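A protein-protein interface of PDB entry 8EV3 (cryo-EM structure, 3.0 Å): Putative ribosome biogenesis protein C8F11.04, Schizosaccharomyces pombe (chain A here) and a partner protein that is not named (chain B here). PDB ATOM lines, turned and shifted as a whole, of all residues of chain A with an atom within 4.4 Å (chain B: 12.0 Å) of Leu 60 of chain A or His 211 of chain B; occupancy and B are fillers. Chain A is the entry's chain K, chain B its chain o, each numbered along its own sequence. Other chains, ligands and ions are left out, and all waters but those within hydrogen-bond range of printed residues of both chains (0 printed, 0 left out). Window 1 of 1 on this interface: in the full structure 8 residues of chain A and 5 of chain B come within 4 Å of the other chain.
Lys 61 of chain A touches His 211 of chain B (CA to NE2, 3.2 Å). CD2 of Phe 62 of chain A touches CB of Arg 208 of chain B, at 3.6 Å. CB of Ser 197 of chain A touches CE1 of His 211 of chain B (3.6 Å).
Of the 11 printed residues of chain A, 4 touch a printed residue of chain B. Hydrophobic or aromatic side chains of chain A that line the printed part of chain B: Phe 62. Among the printed residues, no Asp or Glu carboxylate lies within 4 Å of a Lys or Arg side-chain nitrogen of the other chain.
Of chain B, only His 211 (2.9 Å) comes within 4 Å of Leu 60 of chain A. Printed residues of chain A within 4 Å of His 211 of chain B: Leu 60, Lys 61, Phe 62 and Ser 197. Lys 61 of chain A touches one residue of chain B. Phe 62 of chain A touches just these residues of chain B: Arg 208 and His 211. Of chain B, only His 211 comes within 4 Å of Ser 197 of chain A. Lys 234 of chain A touches none of the printed residues of chain B. Ala 237 of chain A touches none of the printed residues of chain B. No residue of chain B comes within 4 Å of Leu 257 of chain A. Printed residues of chain A within 4 Å of Arg 208 of chain B: Phe 62. Pro 202 of chain B touches none of the printed residues of chain A. Ala 207 of chain B touches none of the printed residues of chain A. The nearest residue of chain B that does not touch Leu 60 of chain A is Glu 212 of chain B (7.4 Å). The nearest printed residue of chain A that does not touch Arg 208 of chain B is Lys 61 of chain A (8.1 Å).
The backbone carbonyl oxygen (O) of Gly 235 of chain A lies within hydrogen-bond range of the backbone NH (N) of Leu 60 of chain A (3.0 Å). N of Thr 59 of chain A is in hydrogen-bond range of O of Ser 197 of chain A (2.8 Å).
NE2 of His 211 of chain B lies within hydrogen-bond range of O of Leu 60 of chain A. N of Phe 62 of chain A sits at hydrogen-bond distance from NE2 of His 211 of chain B.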
ATOM      1  N   ALA A  58      -0.038   0.098  -0.296  1.00  0.00           N
ATOM      2  CA  ALA A  58      -1.410   0.572  -0.407  1.00  0.00           C
ATOM      3  C   ALA A  58      -2.258  -0.125   0.645  1.00  0.00           C
ATOM      4  O   ALA A  58      -2.189  -1.351   0.790  1.00  0.00           O
ATOM      5  CB  ALA A  58      -1.971   0.313  -1.807  1.00  0.00           C
ATOM      6  N   THR A  59      -3.054   0.651   1.374  1.00  0.00           N
ATOM      7  CA  THR A  59      -3.912   0.125   2.424  1.00  0.00           C
ATOM      8  C   THR A  59      -5.374   0.280   2.027  1.00  0.00           C
ATOM      9  O   THR A  59      -5.752   1.238   1.346  1.00  0.00           O
ATOM     10  CB  THR A  59      -3.652   0.832   3.760  1.00  0.00           C
ATOM     11  OG1 THR A  59      -2.246   1.064   3.913  1.00  0.00           O
ATOM     12  CG2 THR A  59      -4.145  -0.016   4.925  1.00  0.00           C
ATOM     13  N   LEU A  60      -6.194  -0.684   2.454  1.00  0.00           N
ATOM     14  CA  LEU A  60      -7.615  -0.649   2.122  1.00  0.00           C
ATOM     15  C   LEU A  60      -8.304   0.572   2.716  1.00  0.00           C
ATOM     16  O   LEU A  60      -9.227   1.123   2.105  1.00  0.00           O
ATOM     17  CB  LEU A  60      -8.298  -1.928   2.605  1.00  0.00           C
ATOM     18  CG  LEU A  60      -7.784  -3.239   2.006  1.00  0.00           C
ATOM     19  CD1 LEU A  60      -8.109  -4.406   2.922  1.00  0.00           C
ATOM     20  CD2 LEU A  60      -8.374  -3.461   0.624  1.00  0.00           C
ATOM     21  N   LYS A  61      -7.872   1.011   3.896  1.00  0.00           N
ATOM     22  CA  LYS A  61      -8.470   2.151   4.573  1.00  0.00           C
ATOM     23  C   LYS A  61      -7.383   3.143   4.961  1.00  0.00           C
ATOM     24  O   LYS A  61      -6.201   2.802   5.040  1.00  0.00           O
ATOM     25  CB  LYS A  61      -9.262   1.718   5.814  1.00  0.00           C
ATOM     26  CG  LYS A  61      -8.404   1.144   6.925  1.00  0.00           C
ATOM     27  CD  LYS A  61      -9.241   0.336   7.901  1.00  0.00           C
ATOM     28  CE  LYS A  61      -8.430  -0.051   9.122  1.00  0.00           C
ATOM     29  NZ  LYS A  61      -7.106  -0.613   8.738  1.00  0.00           N
ATOM     30  N   PHE A  62      -7.804   4.386   5.188  1.00  0.00           N
ATOM     31  CA  PHE A  62      -6.868   5.431   5.580  1.00  0.00           C
ATOM     32  C   PHE A  62      -6.208   5.090   6.912  1.00  0.00           C
ATOM     33  O   PHE A  62      -6.854   4.589   7.836  1.00  0.00           O
ATOM     34  CB  PHE A  62      -7.588   6.778   5.674  1.00  0.00           C
ATOM     35  CG  PHE A  62      -7.579   7.563   4.392  1.00  0.00           C
ATOM     36  CD1 PHE A  62      -7.235   6.959   3.194  1.00  0.00           C
ATOM     37  CD2 PHE A  62      -7.912   8.908   4.386  1.00  0.00           C
ATOM     38  CE1 PHE A  62      -7.226   7.680   2.016  1.00  0.00           C
ATOM     39  CE2 PHE A  62      -7.905   9.634   3.210  1.00  0.00           C
ATOM     40  CZ  PHE A  62      -7.561   9.019   2.024  1.00  0.00           C
ATOM     41  N   SER A 197      -4.048   6.650   1.832  1.00  0.00           N
ATOM     42  CA  SER A 197      -4.092   5.199   1.743  1.00  0.00           C
ATOM     43  C   SER A 197      -2.863   4.601   1.076  1.00  0.00           C
ATOM     44  O   SER A 197      -2.742   3.372   1.030  1.00  0.00           O
ATOM     45  CB  SER A 197      -5.349   4.754   0.979  1.00  0.00           C
ATOM     46  OG  SER A 197      -5.512   5.503  -0.212  1.00  0.00           O
ATOM     47  N   LYS A 234      -3.778  -7.882   7.401  1.00  0.00           N
ATOM     48  CA  LYS A 234      -5.031  -8.200   6.727  1.00  0.00           C
ATOM     49  C   LYS A 234      -5.623  -6.992   6.014  1.00  0.00           C
ATOM     50  O   LYS A 234      -6.362  -7.163   5.039  1.00  0.00           O
ATOM     51  CB  LYS A 234      -6.040  -8.761   7.731  1.00  0.00           C
ATOM     52  N   GLY A 235      -5.317  -5.783   6.474  1.00  0.00           N
ATOM     53  CA  GLY A 235      -5.797  -4.574   5.842  1.00  0.00           C
ATOM     54  C   GLY A 235      -4.964  -4.065   4.691  1.00  0.00           C
ATOM     55  O   GLY A 235      -5.277  -3.011   4.131  1.00  0.00           O
ATOM     56  N   ILE A 236      -3.909  -4.780   4.316  1.00  0.00           N
ATOM     57  CA  ILE A 236      -3.045  -4.352   3.221  1.00  0.00           C
ATOM     58  C   ILE A 236      -3.736  -4.646   1.897  1.00  0.00           C
ATOM     59  O   ILE A 236      -4.154  -5.780   1.638  1.00  0.00           O
ATOM     60  CB  ILE A 236      -1.678  -5.051   3.300  1.00  0.00           C
ATOM     61  CG1 ILE A 236      -0.901  -4.566   4.526  1.00  0.00           C
ATOM     62  CG2 ILE A 236      -0.880  -4.808   2.029  1.00  0.00           C
ATOM     63  CD1 ILE A 236       0.437  -5.247   4.709  1.00  0.00           C
ATOM     64  N   ALA A 237      -3.857  -3.621   1.055  1.00  0.00           N
ATOM     65  CA  ALA A 237      -4.489  -3.775  -0.252  1.00  0.00           C
ATOM     66  C   ALA A 237      -3.506  -4.316  -1.286  1.00  0.00           C
ATOM     67  O   ALA A 237      -3.732  -5.380  -1.872  1.00  0.00           O
ATOM     68  CB  ALA A 237      -5.075  -2.436  -0.712  1.00  0.00           C
ATOM     69  N   LEU A 257      -8.933  -8.591  -1.392  1.00  0.00           N
ATOM     70  CA  LEU A 257      -9.078  -7.162  -1.129  1.00  0.00           C
ATOM     71  C   LEU A 257     -10.428  -6.641  -1.606  1.00  0.00           C
ATOM     72  O   LEU A 257     -11.040  -5.792  -0.945  1.00  0.00           O
ATOM     73  CB  LEU A 257      -7.933  -6.381  -1.783  1.00  0.00           C
ATOM     74  CG  LEU A 257      -7.792  -6.359  -3.308  1.00  0.00           C
ATOM     75  CD1 LEU A 257      -8.449  -5.121  -3.901  1.00  0.00           C
ATOM     76  CD2 LEU A 257      -6.327  -6.418  -3.708  1.00  0.00           C
ATOM     77  N   PRO B 202     -11.228  21.214   3.208  1.00  0.00           N
ATOM     78  CA  PRO B 202     -10.245  20.272   3.770  1.00  0.00           C
ATOM     79  C   PRO B 202     -10.224  18.966   2.982  1.00  0.00           C
ATOM     80  O   PRO B 202     -10.849  17.965   3.329  1.00  0.00           O
ATOM     81  CB  PRO B 202     -10.745  20.084   5.203  1.00  0.00           C
ATOM     82  CG  PRO B 202     -12.228  20.215   5.077  1.00  0.00           C
ATOM     83  CD  PRO B 202     -12.493  21.204   3.963  1.00  0.00           C
ATOM     84  N   HIS B 203      -9.471  18.985   1.880  1.00  0.00           N
ATOM     85  CA  HIS B 203      -9.474  17.863   0.947  1.00  0.00           C
ATOM     86  C   HIS B 203      -9.044  16.562   1.611  1.00  0.00           C
ATOM     87  O   HIS B 203      -9.465  15.481   1.186  1.00  0.00           O
ATOM     88  CB  HIS B 203      -8.560  18.170  -0.237  1.00  0.00           C
ATOM     89  CG  HIS B 203      -9.149  19.126  -1.227  1.00  0.00           C
ATOM     90  ND1 HIS B 203     -10.070  20.090  -0.877  1.00  0.00           N
ATOM     91  CD2 HIS B 203      -8.940  19.270  -2.557  1.00  0.00           C
ATOM     92  CE1 HIS B 203     -10.406  20.784  -1.949  1.00  0.00           C
ATOM     93  NE2 HIS B 203      -9.735  20.307  -2.982  1.00  0.00           N
ATOM     94  N   ALA B 204      -8.203  16.642   2.645  1.00  0.00           N
ATOM     95  CA  ALA B 204      -7.773  15.433   3.338  1.00  0.00           C
ATOM     96  C   ALA B 204      -8.947  14.726   4.004  1.00  0.00           C
ATOM     97  O   ALA B 204      -9.077  13.499   3.911  1.00  0.00           O
ATOM     98  CB  ALA B 204      -6.698  15.775   4.369  1.00  0.00           C
ATOM     99  N   THR B 205      -9.816  15.480   4.680  1.00  0.00           N
ATOM    100  CA  THR B 205     -10.945  14.860   5.367  1.00  0.00           C
ATOM    101  C   THR B 205     -12.027  14.428   4.386  1.00  0.00           C
ATOM    102  O   THR B 205     -12.616  13.352   4.541  1.00  0.00           O
ATOM    103  CB  THR B 205     -11.522  15.814   6.411  1.00  0.00           C
ATOM    104  OG1 THR B 205     -11.459  17.156   5.920  1.00  0.00           O
ATOM    105  CG2 THR B 205     -10.737  15.719   7.710  1.00  0.00           C
ATOM    106  N   ILE B 206     -12.310  15.253   3.372  1.00  0.00           N
ATOM    107  CA  ILE B 206     -13.346  14.892   2.406  1.00  0.00           C
ATOM    108  C   ILE B 206     -12.938  13.653   1.623  1.00  0.00           C
ATOM    109  O   ILE B 206     -13.791  12.850   1.228  1.00  0.00           O
ATOM    110  CB  ILE B 206     -13.673  16.080   1.475  1.00  0.00           C
ATOM    111  CG1 ILE B 206     -12.628  16.229   0.366  1.00  0.00           C
ATOM    112  CG2 ILE B 206     -13.798  17.367   2.273  1.00  0.00           C
ATOM    113  CD1 ILE B 206     -13.131  16.981  -0.846  1.00  0.00           C
ATOM    114  N   ALA B 207     -11.636  13.474   1.382  1.00  0.00           N
ATOM    115  CA  ALA B 207     -11.167  12.218   0.809  1.00  0.00           C
ATOM    116  C   ALA B 207     -11.408  11.063   1.770  1.00  0.00           C
ATOM    117  O   ALA B 207     -11.819   9.976   1.350  1.00  0.00           O
ATOM    118  CB  ALA B 207      -9.686  12.322   0.449  1.00  0.00           C
ATOM    119  N   ARG B 208     -11.162  11.284   3.064  1.00  0.00           N
ATOM    120  CA  ARG B 208     -11.406  10.246   4.060  1.00  0.00           C
ATOM    121  C   ARG B 208     -12.888   9.907   4.160  1.00  0.00           C
ATOM    122  O   ARG B 208     -13.263   8.732   4.245  1.00  0.00           O
ATOM    123  CB  ARG B 208     -10.869  10.689   5.421  1.00  0.00           C
ATOM    124  CG  ARG B 208     -11.634  10.100   6.595  1.00  0.00           C
ATOM    125  CD  ARG B 208     -10.772   9.989   7.832  1.00  0.00           C
ATOM    126  NE  ARG B 208      -9.723  10.999   7.865  1.00  0.00           N
ATOM    127  CZ  ARG B 208      -8.832  11.110   8.839  1.00  0.00           C
ATOM    128  NH1 ARG B 208      -8.850  10.299   9.883  1.00  0.00           N
ATOM    129  NH2 ARG B 208      -7.905  12.060   8.766  1.00  0.00           N
ATOM    130  N   LEU B 209     -13.748  10.929   4.157  1.00  0.00           N
ATOM    131  CA  LEU B 209     -15.183  10.688   4.281  1.00  0.00           C
ATOM    132  C   LEU B 209     -15.687   9.810   3.146  1.00  0.00           C
ATOM    133  O   LEU B 209     -16.424   8.843   3.372  1.00  0.00           O
ATOM    134  CB  LEU B 209     -15.946  12.013   4.300  1.00  0.00           C
ATOM    135  CG  LEU B 209     -16.226  12.693   5.641  1.00  0.00           C
ATOM    136  CD1 LEU B 209     -15.057  12.556   6.607  1.00  0.00           C
ATOM    137  CD2 LEU B 209     -16.570  14.147   5.398  1.00  0.00           C
ATOM    138  N   GLN B 210     -15.295  10.133   1.915  1.00  0.00           N
ATOM    139  CA  GLN B 210     -15.638   9.277   0.788  1.00  0.00           C
ATOM    140  C   GLN B 210     -14.887   7.953   0.850  1.00  0.00           C
ATOM    141  O   GLN B 210     -15.411   6.923   0.413  1.00  0.00           O
ATOM    142  CB  GLN B 210     -15.352  10.008  -0.521  1.00  0.00           C
ATOM    143  CG  GLN B 210     -16.098  11.321  -0.675  1.00  0.00           C
ATOM    144  CD  GLN B 210     -15.368  12.300  -1.571  1.00  0.00           C
ATOM    145  OE1 GLN B 210     -14.313  11.985  -2.122  1.00  0.00           O
ATOM    146  NE2 GLN B 210     -15.926  13.494  -1.724  1.00  0.00           N
ATOM    147  N   HIS B 211     -13.660   7.962   1.381  1.00  0.00           N
ATOM    148  CA  HIS B 211     -12.942   6.712   1.609  1.00  0.00           C
ATOM    149  C   HIS B 211     -13.671   5.836   2.619  1.00  0.00           C
ATOM    150  O   HIS B 211     -13.799   4.621   2.425  1.00  0.00           O
ATOM    151  CB  HIS B 211     -11.519   7.000   2.088  1.00  0.00           C
ATOM    152  CG  HIS B 211     -10.585   5.840   1.951  1.00  0.00           C
ATOM    153  ND1 HIS B 211      -9.650   5.752   0.941  1.00  0.00           N
ATOM    154  CD2 HIS B 211     -10.443   4.716   2.692  1.00  0.00           C
ATOM    155  CE1 HIS B 211      -8.968   4.629   1.071  1.00  0.00           C
ATOM    156  NE2 HIS B 211      -9.433   3.980   2.123  1.00  0.00           N
ATOM    157  N   GLU B 212     -14.154   6.435   3.704  1.00  0.00           N
ATOM    158  CA  GLU B 212     -14.884   5.714   4.738  1.00  0.00           C
ATOM    159  C   GLU B 212     -16.375   5.617   4.451  1.00  0.00           C
ATOM    160  O   GLU B 212     -17.100   4.991   5.230  1.00  0.00           O
ATOM    161  CB  GLU B 212     -14.663   6.380   6.099  1.00  0.00           C
ATOM    162  N   LYS B 213     -16.848   6.223   3.367  1.00  0.00           N
ATOM    163  CA  LYS B 213     -18.255   6.120   3.018  1.00  0.00           C
ATOM    164  C   LYS B 213     -18.596   4.674   2.669  1.00  0.00           C
ATOM    165  O   LYS B 213     -17.783   3.977   2.049  1.00  0.00           O
ATOM    166  CB  LYS B 213     -18.590   7.037   1.841  1.00  0.00           C
ATOM    167  N   PRO B 214     -19.772   4.187   3.061  1.00  0.00           N
ATOM    168  CA  PRO B 214     -20.133   2.801   2.742  1.00  0.00           C
ATOM    169  C   PRO B 214     -20.189   2.574   1.239  1.00  0.00           C
ATOM    170  O   PRO B 214     -20.638   3.432   0.475  1.00  0.00           O
ATOM    171  CB  PRO B 214     -21.511   2.636   3.390  1.00  0.00           C
ATOM    172  N   LEU B 215     -19.725   1.400   0.819  1.00  0.00           N
ATOM    173  CA  LEU B 215     -19.726   1.000  -0.583  1.00  0.00           C
ATOM    174  C   LEU B 215     -20.413  -0.352  -0.697  1.00  0.00           C
ATOM    175  O   LEU B 215     -20.027  -1.308  -0.016  1.00  0.00           O
ATOM    176  CB  LEU B 215     -18.302   0.933  -1.138  1.00  0.00           C
ATOM    177  N   SER B 216     -21.427  -0.430  -1.554  1.00  0.00           N
ATOM    178  CA  SER B 216     -22.161  -1.667  -1.746  1.00  0.00           C
ATOM    179  C   SER B 216     -21.370  -2.628  -2.631  1.00  0.00           C
ATOM    180  O   SER B 216     -20.281  -2.315  -3.122  1.00  0.00           O
ATOM    181  CB  SER B 216     -23.533  -1.386  -2.357  1.00  0.00           C
ATOM    182  N   LYS B 219     -21.188  -1.117  -5.961  1.00  0.00           N
ATOM    183  CA  LYS B 219     -20.199  -0.046  -5.908  1.00  0.00           C
ATOM    184  C   LYS B 219     -18.783  -0.607  -5.874  1.00  0.00           C
ATOM    185  O   LYS B 219     -17.881  -0.078  -6.532  1.00  0.00           O
ATOM    186  CB  LYS B 219     -20.455   0.846  -4.694  1.00  0.00           C
ATOM    187  N   ALA B 220     -18.570  -1.679  -5.105  1.00  0.00           N
ATOM    188  CA  ALA B 220     -17.258  -2.318  -5.073  1.00  0.00           C
ATOM    189  C   ALA B 220     -16.903  -2.912  -6.428  1.00  0.00           C
ATOM    190  O   ALA B 220     -15.747  -2.841  -6.862  1.00  0.00           O
ATOM    191  CB  ALA B 220     -17.223  -3.392  -3.986  1.00  0.00           C
ATOM    192  N   LEU B 223     -15.976  -0.086  -8.334  1.00  0.00           N
ATOM    193  CA  LEU B 223     -14.669   0.335  -7.841  1.00  0.00           C
ATOM    194  C   LEU B 223     -13.564  -0.578  -8.356  1.00  0.00           C
ATOM    195  O   LEU B 223     -12.472  -0.111  -8.699  1.00  0.00           O
ATOM    196  CB  LEU B 223     -14.670   0.368  -6.312  1.00  0.00           C
ATOM    197  N   ILE B 224     -13.826  -1.887  -8.406  1.00  0.00           N
ATOM    198  CA  ILE B 224     -12.846  -2.820  -8.956  1.00  0.00           C
ATOM    199  C   ILE B 224     -12.600  -2.516 -10.429  1.00  0.00           C
ATOM    200  O   ILE B 224     -11.452  -2.427 -10.879  1.00  0.00           O
ATOM    201  CB  ILE B 224     -13.309  -4.272  -8.748  1.00  0.00           C
ATOM    202  N   HIS B 227      -9.286  -3.029 -12.661  1.00  0.00           N
ATOM    203  CA  HIS B 227      -8.043  -3.063 -11.898  1.00  0.00           C
ATOM    204  C   HIS B 227      -7.236  -4.313 -12.220  1.00  0.00           C
ATOM    205  O   HIS B 227      -6.010  -4.247 -12.373  1.00  0.00           O
ATOM    206  CB  HIS B 227      -8.339  -2.985 -10.401  1.00  0.00           C
